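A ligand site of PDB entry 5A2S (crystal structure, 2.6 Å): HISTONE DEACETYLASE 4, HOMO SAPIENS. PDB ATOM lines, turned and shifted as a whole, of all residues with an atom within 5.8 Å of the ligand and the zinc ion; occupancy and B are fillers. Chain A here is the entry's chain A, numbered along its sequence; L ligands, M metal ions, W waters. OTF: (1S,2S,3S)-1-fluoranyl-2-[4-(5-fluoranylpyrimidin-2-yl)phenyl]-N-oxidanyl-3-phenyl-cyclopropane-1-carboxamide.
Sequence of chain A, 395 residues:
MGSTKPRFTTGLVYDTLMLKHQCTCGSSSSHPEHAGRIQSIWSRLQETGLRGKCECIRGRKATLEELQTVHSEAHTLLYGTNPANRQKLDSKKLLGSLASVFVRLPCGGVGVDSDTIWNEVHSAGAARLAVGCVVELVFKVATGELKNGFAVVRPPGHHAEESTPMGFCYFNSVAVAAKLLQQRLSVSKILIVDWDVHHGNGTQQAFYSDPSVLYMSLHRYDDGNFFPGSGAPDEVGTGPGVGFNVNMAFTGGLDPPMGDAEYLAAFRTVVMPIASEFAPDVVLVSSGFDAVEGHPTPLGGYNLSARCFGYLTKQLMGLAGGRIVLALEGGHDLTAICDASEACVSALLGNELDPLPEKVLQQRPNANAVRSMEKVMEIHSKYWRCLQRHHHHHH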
ATOM      1  N   PRO A  32       5.758 -18.755  15.503  1.00  0.00           N
ATOM      2  CA  PRO A  32       5.354 -20.171  15.435  1.00  0.00           C
ATOM      3  C   PRO A  32       6.289 -21.083  14.653  1.00  0.00           C
ATOM      4  O   PRO A  32       6.531 -22.193  15.090  1.00  0.00           O
ATOM      5  CB  PRO A  32       3.980 -20.123  14.752  1.00  0.00           C
ATOM      6  CG  PRO A  32       3.527 -18.703  14.825  1.00  0.00           C
ATOM      7  CD  PRO A  32       4.758 -17.863  14.897  1.00  0.00           C
ATOM      8  N   GLU A  33       6.804 -20.654  13.506  1.00  0.00           N
ATOM      9  CA  GLU A  33       7.735 -21.490  12.739  1.00  0.00           C
ATOM     10  C   GLU A  33       9.102 -21.395  13.409  1.00  0.00           C
ATOM     11  O   GLU A  33       9.899 -20.526  13.056  1.00  0.00           O
ATOM     12  CB  GLU A  33       7.786 -21.048  11.263  1.00  0.00           C
ATOM     13  CG  GLU A  33       8.310 -22.090  10.275  1.00  0.00           C
ATOM     14  CD  GLU A  33       9.810 -22.348  10.391  1.00  0.00           C
ATOM     15  OE1 GLU A  33      10.607 -21.487   9.940  1.00  0.00           O
ATOM     16  OE2 GLU A  33      10.188 -23.410  10.925  1.00  0.00           O
ATOM     17  N   HIS A  34       9.375 -22.269  14.366  1.00  0.00           N
ATOM     18  CA  HIS A  34      10.595 -22.161  15.206  1.00  0.00           C
ATOM     19  C   HIS A  34      11.557 -23.318  15.108  1.00  0.00           C
ATOM     20  O   HIS A  34      11.190 -24.435  14.773  1.00  0.00           O
ATOM     21  CB  HIS A  34      10.215 -21.931  16.662  1.00  0.00           C
ATOM     22  CG  HIS A  34       9.485 -23.091  17.299  1.00  0.00           C
ATOM     23  ND1 HIS A  34      10.069 -23.909  18.185  1.00  0.00           N
ATOM     24  CD2 HIS A  34       8.188 -23.555  17.134  1.00  0.00           C
ATOM     25  CE1 HIS A  34       9.185 -24.848  18.584  1.00  0.00           C
ATOM     26  NE2 HIS A  34       8.032 -24.631  17.923  1.00  0.00           N
ATOM     27  N   ARG A  37      10.969 -26.951  16.139  1.00  0.00           N
ATOM     28  CA  ARG A  37      10.133 -27.835  15.319  1.00  0.00           C
ATOM     29  C   ARG A  37      10.918 -28.989  14.709  1.00  0.00           C
ATOM     30  O   ARG A  37      10.631 -30.147  15.010  1.00  0.00           O
ATOM     31  CB  ARG A  37       9.423 -27.033  14.217  1.00  0.00           C
ATOM     32  CG  ARG A  37       8.400 -26.024  14.736  1.00  0.00           C
ATOM     33  CD  ARG A  37       7.833 -25.159  13.624  1.00  0.00           C
ATOM     34  NE  ARG A  37       7.123 -25.958  12.634  1.00  0.00           N
ATOM     35  CZ  ARG A  37       7.582 -26.286  11.430  1.00  0.00           C
ATOM     36  NH1 ARG A  37       8.774 -25.883  10.994  1.00  0.00           N
ATOM     37  NH2 ARG A  37       6.828 -27.031  10.625  1.00  0.00           N
ATOM     38  N   ASP A 115       4.592 -10.180   9.456  1.00  0.00           N
ATOM     39  CA  ASP A 115       4.941 -11.310  10.326  1.00  0.00           C
ATOM     40  C   ASP A 115       6.011 -12.312   9.832  1.00  0.00           C
ATOM     41  O   ASP A 115       6.423 -13.170  10.623  1.00  0.00           O
ATOM     42  CB  ASP A 115       3.666 -12.063  10.725  1.00  0.00           C
ATOM     43  CG  ASP A 115       2.773 -12.359   9.556  1.00  0.00           C
ATOM     44  OD1 ASP A 115       3.330 -12.671   8.481  1.00  0.00           O
ATOM     45  OD2 ASP A 115       1.530 -12.273   9.700  1.00  0.00           O
ATOM     46  N   PRO A 156       9.712 -23.421   5.770  1.00  0.00           N
ATOM     47  CA  PRO A 156       8.820 -24.051   4.786  1.00  0.00           C
ATOM     48  C   PRO A 156       8.844 -23.333   3.439  1.00  0.00           C
ATOM     49  O   PRO A 156       9.437 -22.273   3.327  1.00  0.00           O
ATOM     50  CB  PRO A 156       7.437 -23.957   5.430  1.00  0.00           C
ATOM     51  CG  PRO A 156       7.543 -22.838   6.409  1.00  0.00           C
ATOM     52  CD  PRO A 156       8.965 -22.793   6.875  1.00  0.00           C
ATOM     53  N   HIS A 158       5.935 -23.934   0.439  1.00  0.00           N
ATOM     54  CA  HIS A 158       4.800 -23.959  -0.510  1.00  0.00           C
ATOM     55  C   HIS A 158       3.993 -22.682  -0.680  1.00  0.00           C
ATOM     56  O   HIS A 158       3.141 -22.616  -1.555  1.00  0.00           O
ATOM     57  CB  HIS A 158       3.879 -25.168  -0.234  1.00  0.00           C
ATOM     58  CG  HIS A 158       3.070 -25.070   1.047  1.00  0.00           C
ATOM     59  ND1 HIS A 158       1.842 -25.613   1.159  1.00  0.00           N
ATOM     60  CD2 HIS A 158       3.341 -24.472   2.275  1.00  0.00           C
ATOM     61  CE1 HIS A 158       1.350 -25.381   2.396  1.00  0.00           C
ATOM     62  NE2 HIS A 158       2.270 -24.670   3.071  1.00  0.00           N
ATOM     63  N   HIS A 159       4.265 -21.658   0.128  1.00  0.00           N
ATOM     64  CA  HIS A 159       3.623 -20.353  -0.040  1.00  0.00           C
ATOM     65  C   HIS A 159       4.496 -19.400  -0.804  1.00  0.00           C
ATOM     66  O   HIS A 159       4.029 -18.319  -1.168  1.00  0.00           O
ATOM     67  CB  HIS A 159       3.312 -19.714   1.313  1.00  0.00           C
ATOM     68  CG  HIS A 159       2.277 -20.450   2.118  1.00  0.00           C
ATOM     69  ND1 HIS A 159       1.058 -20.746   1.644  1.00  0.00           N
ATOM     70  CD2 HIS A 159       2.296 -20.892   3.439  1.00  0.00           C
ATOM     71  CE1 HIS A 159       0.346 -21.368   2.591  1.00  0.00           C
ATOM     72  NE2 HIS A 159       1.110 -21.453   3.691  1.00  0.00           N
ATOM     73  N   GLY A 167       3.919 -16.303   4.459  1.00  0.00           N
ATOM     74  CA  GLY A 167       3.709 -17.434   5.368  1.00  0.00           C
ATOM     75  C   GLY A 167       4.991 -18.126   5.788  1.00  0.00           C
ATOM     76  O   GLY A 167       5.098 -19.347   5.724  1.00  0.00           O
ATOM     77  N   PHE A 168       5.980 -17.336   6.203  1.00  0.00           N
ATOM     78  CA  PHE A 168       7.264 -17.851   6.673  1.00  0.00           C
ATOM     79  C   PHE A 168       8.048 -18.642   5.631  1.00  0.00           C
ATOM     80  O   PHE A 168       8.992 -19.367   5.989  1.00  0.00           O
ATOM     81  CB  PHE A 168       7.064 -18.732   7.909  1.00  0.00           C
ATOM     82  CG  PHE A 168       6.164 -18.131   8.957  1.00  0.00           C
ATOM     83  CD1 PHE A 168       6.174 -16.768   9.225  1.00  0.00           C
ATOM     84  CD2 PHE A 168       5.342 -18.946   9.715  1.00  0.00           C
ATOM     85  CE1 PHE A 168       5.348 -16.236  10.200  1.00  0.00           C
ATOM     86  CE2 PHE A 168       4.524 -18.419  10.693  1.00  0.00           C
ATOM     87  CZ  PHE A 168       4.523 -17.053  10.934  1.00  0.00           C
ATOM     88  N   CYS A 169       7.674 -18.497   4.353  1.00  0.00           N
ATOM     89  CA  CYS A 169       8.372 -19.171   3.254  1.00  0.00           C
ATOM     90  C   CYS A 169       9.089 -18.149   2.393  1.00  0.00           C
ATOM     91  O   CYS A 169       8.625 -17.023   2.240  1.00  0.00           O
ATOM     92  CB  CYS A 169       7.408 -19.954   2.383  1.00  0.00           C
ATOM     93  SG  CYS A 169       6.315 -21.060   3.269  1.00  0.00           S
ATOM     94  N   ASP A 196      -0.604 -30.429   3.710  1.00  0.00           N
ATOM     95  CA  ASP A 196      -0.634 -29.350   4.691  1.00  0.00           C
ATOM     96  C   ASP A 196      -2.034 -28.725   4.687  1.00  0.00           C
ATOM     97  O   ASP A 196      -2.731 -28.722   3.657  1.00  0.00           O
ATOM     98  CB  ASP A 196       0.417 -28.280   4.340  1.00  0.00           C
ATOM     99  CG  ASP A 196       0.481 -27.162   5.379  1.00  0.00           C
ATOM    100  OD1 ASP A 196      -0.392 -26.275   5.425  1.00  0.00           O
ATOM    101  OD2 ASP A 196       1.448 -27.167   6.157  1.00  0.00           O
ATOM    102  N   VAL A 197      -2.441 -28.199   5.835  1.00  0.00           N
ATOM    103  CA  VAL A 197      -3.806 -27.745   6.032  1.00  0.00           C
ATOM    104  C   VAL A 197      -4.077 -26.508   5.193  1.00  0.00           C
ATOM    105  O   VAL A 197      -5.217 -26.248   4.807  1.00  0.00           O
ATOM    106  CB  VAL A 197      -4.101 -27.466   7.526  1.00  0.00           C
ATOM    107  CG1 VAL A 197      -3.670 -26.061   7.926  1.00  0.00           C
ATOM    108  CG2 VAL A 197      -5.574 -27.697   7.838  1.00  0.00           C
ATOM    109  N   HIS A 198      -3.015 -25.764   4.901  1.00  0.00           N
ATOM    110  CA  HIS A 198      -3.115 -24.554   4.108  1.00  0.00           C
ATOM    111  C   HIS A 198      -2.826 -24.874   2.676  1.00  0.00           C
ATOM    112  O   HIS A 198      -2.032 -25.767   2.386  1.00  0.00           O
ATOM    113  CB  HIS A 198      -2.125 -23.514   4.604  1.00  0.00           C
ATOM    114  CG  HIS A 198      -2.266 -23.186   6.070  1.00  0.00           C
ATOM    115  ND1 HIS A 198      -1.484 -23.741   7.007  1.00  0.00           N
ATOM    116  CD2 HIS A 198      -3.131 -22.334   6.747  1.00  0.00           C
ATOM    117  CE1 HIS A 198      -1.825 -23.269   8.216  1.00  0.00           C
ATOM    118  NE2 HIS A 198      -2.837 -22.408   8.057  1.00  0.00           N
ATOM    119  N   PHE A 227      -6.271 -18.847   5.575  1.00  0.00           N
ATOM    120  CA  PHE A 227      -4.972 -18.530   4.997  1.00  0.00           C
ATOM    121  C   PHE A 227      -4.525 -19.681   4.086  1.00  0.00           C
ATOM    122  O   PHE A 227      -4.714 -20.848   4.418  1.00  0.00           O
ATOM    123  CB  PHE A 227      -3.938 -18.280   6.102  1.00  0.00           C
ATOM    124  CG  PHE A 227      -2.574 -17.835   5.616  1.00  0.00           C
ATOM    125  CD1 PHE A 227      -1.588 -18.758   5.320  1.00  0.00           C
ATOM    126  CD2 PHE A 227      -2.272 -16.479   5.489  1.00  0.00           C
ATOM    127  CE1 PHE A 227      -0.331 -18.355   4.887  1.00  0.00           C
ATOM    128  CE2 PHE A 227      -1.023 -16.071   5.053  1.00  0.00           C
ATOM    129  CZ  PHE A 227      -0.058 -17.005   4.756  1.00  0.00           C
ATOM    130  N   ASP A 290      -0.333 -29.567  10.039  1.00  0.00           N
ATOM    131  CA  ASP A 290      -1.290 -28.727  10.779  1.00  0.00           C
ATOM    132  C   ASP A 290      -2.764 -29.189  10.720  1.00  0.00           C
ATOM    133  O   ASP A 290      -3.618 -28.620  11.407  1.00  0.00           O
ATOM    134  CB  ASP A 290      -1.145 -27.239  10.397  1.00  0.00           C
ATOM    135  CG  ASP A 290      -0.665 -27.032   8.994  1.00  0.00           C
ATOM    136  OD1 ASP A 290      -0.812 -27.961   8.152  1.00  0.00           O
ATOM    137  OD2 ASP A 290      -0.138 -25.925   8.723  1.00  0.00           O
ATOM    138  N   PRO A 298      -5.959 -19.688  13.548  1.00  0.00           N
ATOM    139  CA  PRO A 298      -5.900 -19.916  12.103  1.00  0.00           C
ATOM    140  C   PRO A 298      -4.862 -20.935  11.682  1.00  0.00           C
ATOM    141  O   PRO A 298      -4.652 -21.152  10.478  1.00  0.00           O
ATOM    142  CB  PRO A 298      -5.492 -18.532  11.581  1.00  0.00           C
ATOM    143  CG  PRO A 298      -4.591 -18.013  12.629  1.00  0.00           C
ATOM    144  CD  PRO A 298      -5.169 -18.506  13.931  1.00  0.00           C
ATOM    145  N   LEU A 299      -4.198 -21.556  12.653  1.00  0.00           N
ATOM    146  CA  LEU A 299      -3.150 -22.517  12.392  1.00  0.00           C
ATOM    147  C   LEU A 299      -3.741 -23.787  11.774  1.00  0.00           C
ATOM    148  O   LEU A 299      -3.130 -24.393  10.894  1.00  0.00           O
ATOM    149  CB  LEU A 299      -2.392 -22.838  13.675  1.00  0.00           C
ATOM    150  CG  LEU A 299      -0.860 -22.763  13.680  1.00  0.00           C
ATOM    151  CD1 LEU A 299      -0.372 -21.398  13.214  1.00  0.00           C
ATOM    152  CD2 LEU A 299      -0.348 -23.062  15.078  1.00  0.00           C
ATOM    153  N   GLU A 329       6.510 -29.139   5.681  1.00  0.00           N
ATOM    154  CA  GLU A 329       5.992 -27.790   5.429  1.00  0.00           C
ATOM    155  C   GLU A 329       5.536 -27.243   6.778  1.00  0.00           C
ATOM    156  O   GLU A 329       6.364 -27.020   7.652  1.00  0.00           O
ATOM    157  CB  GLU A 329       4.878 -27.803   4.389  1.00  0.00           C
ATOM    158  CG  GLU A 329       5.268 -28.390   3.032  1.00  0.00           C
ATOM    159  CD  GLU A 329       6.048 -27.435   2.125  1.00  0.00           C
ATOM    160  OE1 GLU A 329       6.310 -26.285   2.515  1.00  0.00           O
ATOM    161  OE2 GLU A 329       6.394 -27.856   0.990  1.00  0.00           O
ATOM    162  N   GLY A 330       4.223 -27.033   6.960  1.00  0.00           N
ATOM    163  CA  GLY A 330       3.672 -26.577   8.255  1.00  0.00           C
ATOM    164  C   GLY A 330       3.502 -27.681   9.292  1.00  0.00           C
ATOM    165  O   GLY A 330       3.758 -28.866   9.017  1.00  0.00           O
ATOM    166  N   GLY A 331       3.035 -27.286  10.480  1.00  0.00           N
ATOM    167  CA  GLY A 331       2.945 -28.184  11.648  1.00  0.00           C
ATOM    168  C   GLY A 331       3.584 -27.486  12.838  1.00  0.00           C
ATOM    169  O   GLY A 331       4.696 -26.978  12.721  1.00  0.00           O
ATOM    170  N   HIS A 332       2.903 -27.480  13.979  1.00  0.00           N
ATOM    171  CA  HIS A 332       3.279 -26.611  15.121  1.00  0.00           C
ATOM    172  C   HIS A 332       3.343 -27.337  16.435  1.00  0.00           C
ATOM    173  O   HIS A 332       4.344 -27.232  17.142  1.00  0.00           O
ATOM    174  CB  HIS A 332       2.300 -25.446  15.242  1.00  0.00           C
ATOM    175  CG  HIS A 332       2.589 -24.534  16.415  1.00  0.00           C
ATOM    176  ND1 HIS A 332       1.894 -24.597  17.563  1.00  0.00           N
ATOM    177  CD2 HIS A 332       3.530 -23.530  16.582  1.00  0.00           C
ATOM    178  CE1 HIS A 332       2.373 -23.685  18.431  1.00  0.00           C
ATOM    179  NE2 HIS A 332       3.372 -23.021  17.823  1.00  0.00           N
HETATM  180  C1  OTF L   1       1.589 -22.862   7.483  1.00  0.00           C
HETATM  181  C2  OTF L   1       1.777 -21.424   7.922  1.00  0.00           C
HETATM  182  C3  OTF L   1       1.189 -20.925   9.253  1.00  0.00           C
HETATM  183  C4  OTF L   1       2.702 -20.987   9.047  1.00  0.00           C
HETATM  184  F5  OTF L   1       1.838 -20.534   6.950  1.00  0.00           F
HETATM  185  O6  OTF L   1       1.212 -23.800   8.167  1.00  0.00           O
HETATM  186  N7  OTF L   1       1.807 -22.970   6.175  1.00  0.00           N
HETATM  187  O8  OTF L   1       1.526 -24.133   5.458  1.00  0.00           O
HETATM  188  C9  OTF L   1       3.417 -21.945   9.911  1.00  0.00           C
HETATM  189  C10 OTF L   1       3.244 -21.861  11.284  1.00  0.00           C
HETATM  190  C11 OTF L   1       3.942 -22.718  12.119  1.00  0.00           C
HETATM  191  C12 OTF L   1       4.827 -23.641  11.577  1.00  0.00           C
HETATM  192  C13 OTF L   1       5.014 -23.708  10.201  1.00  0.00           C
HETATM  193  C14 OTF L   1       4.316 -22.851   9.366  1.00  0.00           C
HETATM  194  C15 OTF L   1       0.456 -19.630   9.095  1.00  0.00           C
HETATM  195  C16 OTF L   1       1.086 -18.388   9.022  1.00  0.00           C
HETATM  196  C17 OTF L   1       0.357 -17.216   8.860  1.00  0.00           C
HETATM  197  C18 OTF L   1      -1.030 -17.257   8.766  1.00  0.00           C
HETATM  198  C19 OTF L   1      -1.663 -18.495   8.822  1.00  0.00           C
HETATM  199  C20 OTF L   1      -0.933 -19.661   8.992  1.00  0.00           C
HETATM  200  C21 OTF L   1      -1.819 -16.006   8.574  1.00  0.00           C
HETATM  201  N22 OTF L   1      -3.162 -15.994   8.820  1.00  0.00           N
HETATM  202  C23 OTF L   1      -3.882 -14.882   8.628  1.00  0.00           C
HETATM  203  C24 OTF L   1      -3.242 -13.727   8.154  1.00  0.00           C
HETATM  204  C25 OTF L   1      -1.872 -13.763   7.897  1.00  0.00           C
HETATM  205  N26 OTF L   1      -1.201 -14.897   8.102  1.00  0.00           N
HETATM  206  F27 OTF L   1      -3.933 -12.598   7.957  1.00  0.00           F
HETATM  207 ZN    ZN M   1       0.217 -25.044   6.937  1.00  0.00          ZN
HETATM  208  O   HOH W   1       1.770 -25.212  10.901  1.00  0.00           O
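CB of Pro 32 touches C11 of the ligand (3.7 Å).
Glu 33 touches the ligand.
NE of Arg 37 touches C12 of the ligand, at 3.4 Å.
Gly 167 touches the ligand (O to F5, 3.7 Å).
Phe 168 touches the ligand (CD2 to C4, 3.4 Å).
CD2 of Phe 227 touches C21 of the ligand, at 3.2 Å.
Gly 330 touches the ligand (CA to O6, 3.7 Å).
O of Gly 331 touches C12 of the ligand, 3.5 Å away.
Hydrophobic or aromatic side chains within 4 Å of the ligand: Pro 32, His 158, His 159, Phe 168, His 198 and Phe 227.
13 residues have an atom within 4 Å of the ligand: Pro 32, Glu 33, Arg 37, His 158, His 159, Gly 167, Phe 168, Asp 196, His 198, Phe 227, Asp 290, Gly 330 and Gly 331.
An oxygen (O8) of the ligand sits close to a ring nitrogen (NE2) of His 158, at 2.6 Å.
A nitrogen (N7) of the ligand is in hydrogen-bond range of a ring nitrogen (NE2) of His 159, at 3.0 Å.
The zinc ion is bound by O6 of the ligand (2.0 Å), OD2 of Asp 290 (2.0 Å), OD1 of Asp 196 (2.0 Å), ND1 of His 198 (2.1 Å), O8 of the ligand (2.2 Å) and OD2 of Asp 196 (2.6 Å).
Three residues have an atom within 4 Å of the zinc ion: Asp 196, His 198 and Asp 290.
The side-chain carboxylate (OD1) of Asp 290 sits at hydrogen-bond distance from the backbone NH (N) of Val 197.
The side-chain carboxylate (OD2) of Asp 196 sits close to the backbone NH (N) of Gly 330, 2.9 Å away.
NE2 of His 198 sits close to O of Leu 299, 3.5 Å away.
The backbone carbonyl oxygen (O) of Pro 298 is in hydrogen-bond range of a ring nitrogen (NE2) of His 198 (3.3 Å).
The backbone NH (N) of His 158 lies within hydrogen-bond range of the side-chain carboxylate (OE1) of Glu 329 (3.2 Å).
O of Gly 331 sits at hydrogen-bond distance from NE of Arg 37, 2.6 Å away.
NH2 of Arg 37 is in hydrogen-bond range of O of Glu 329 (3.0 Å).
The side-chain sulfur of Cys 169 sits at hydrogen-bond distance from the backbone carbonyl oxygen of Gly 167, 3.2 Å away.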
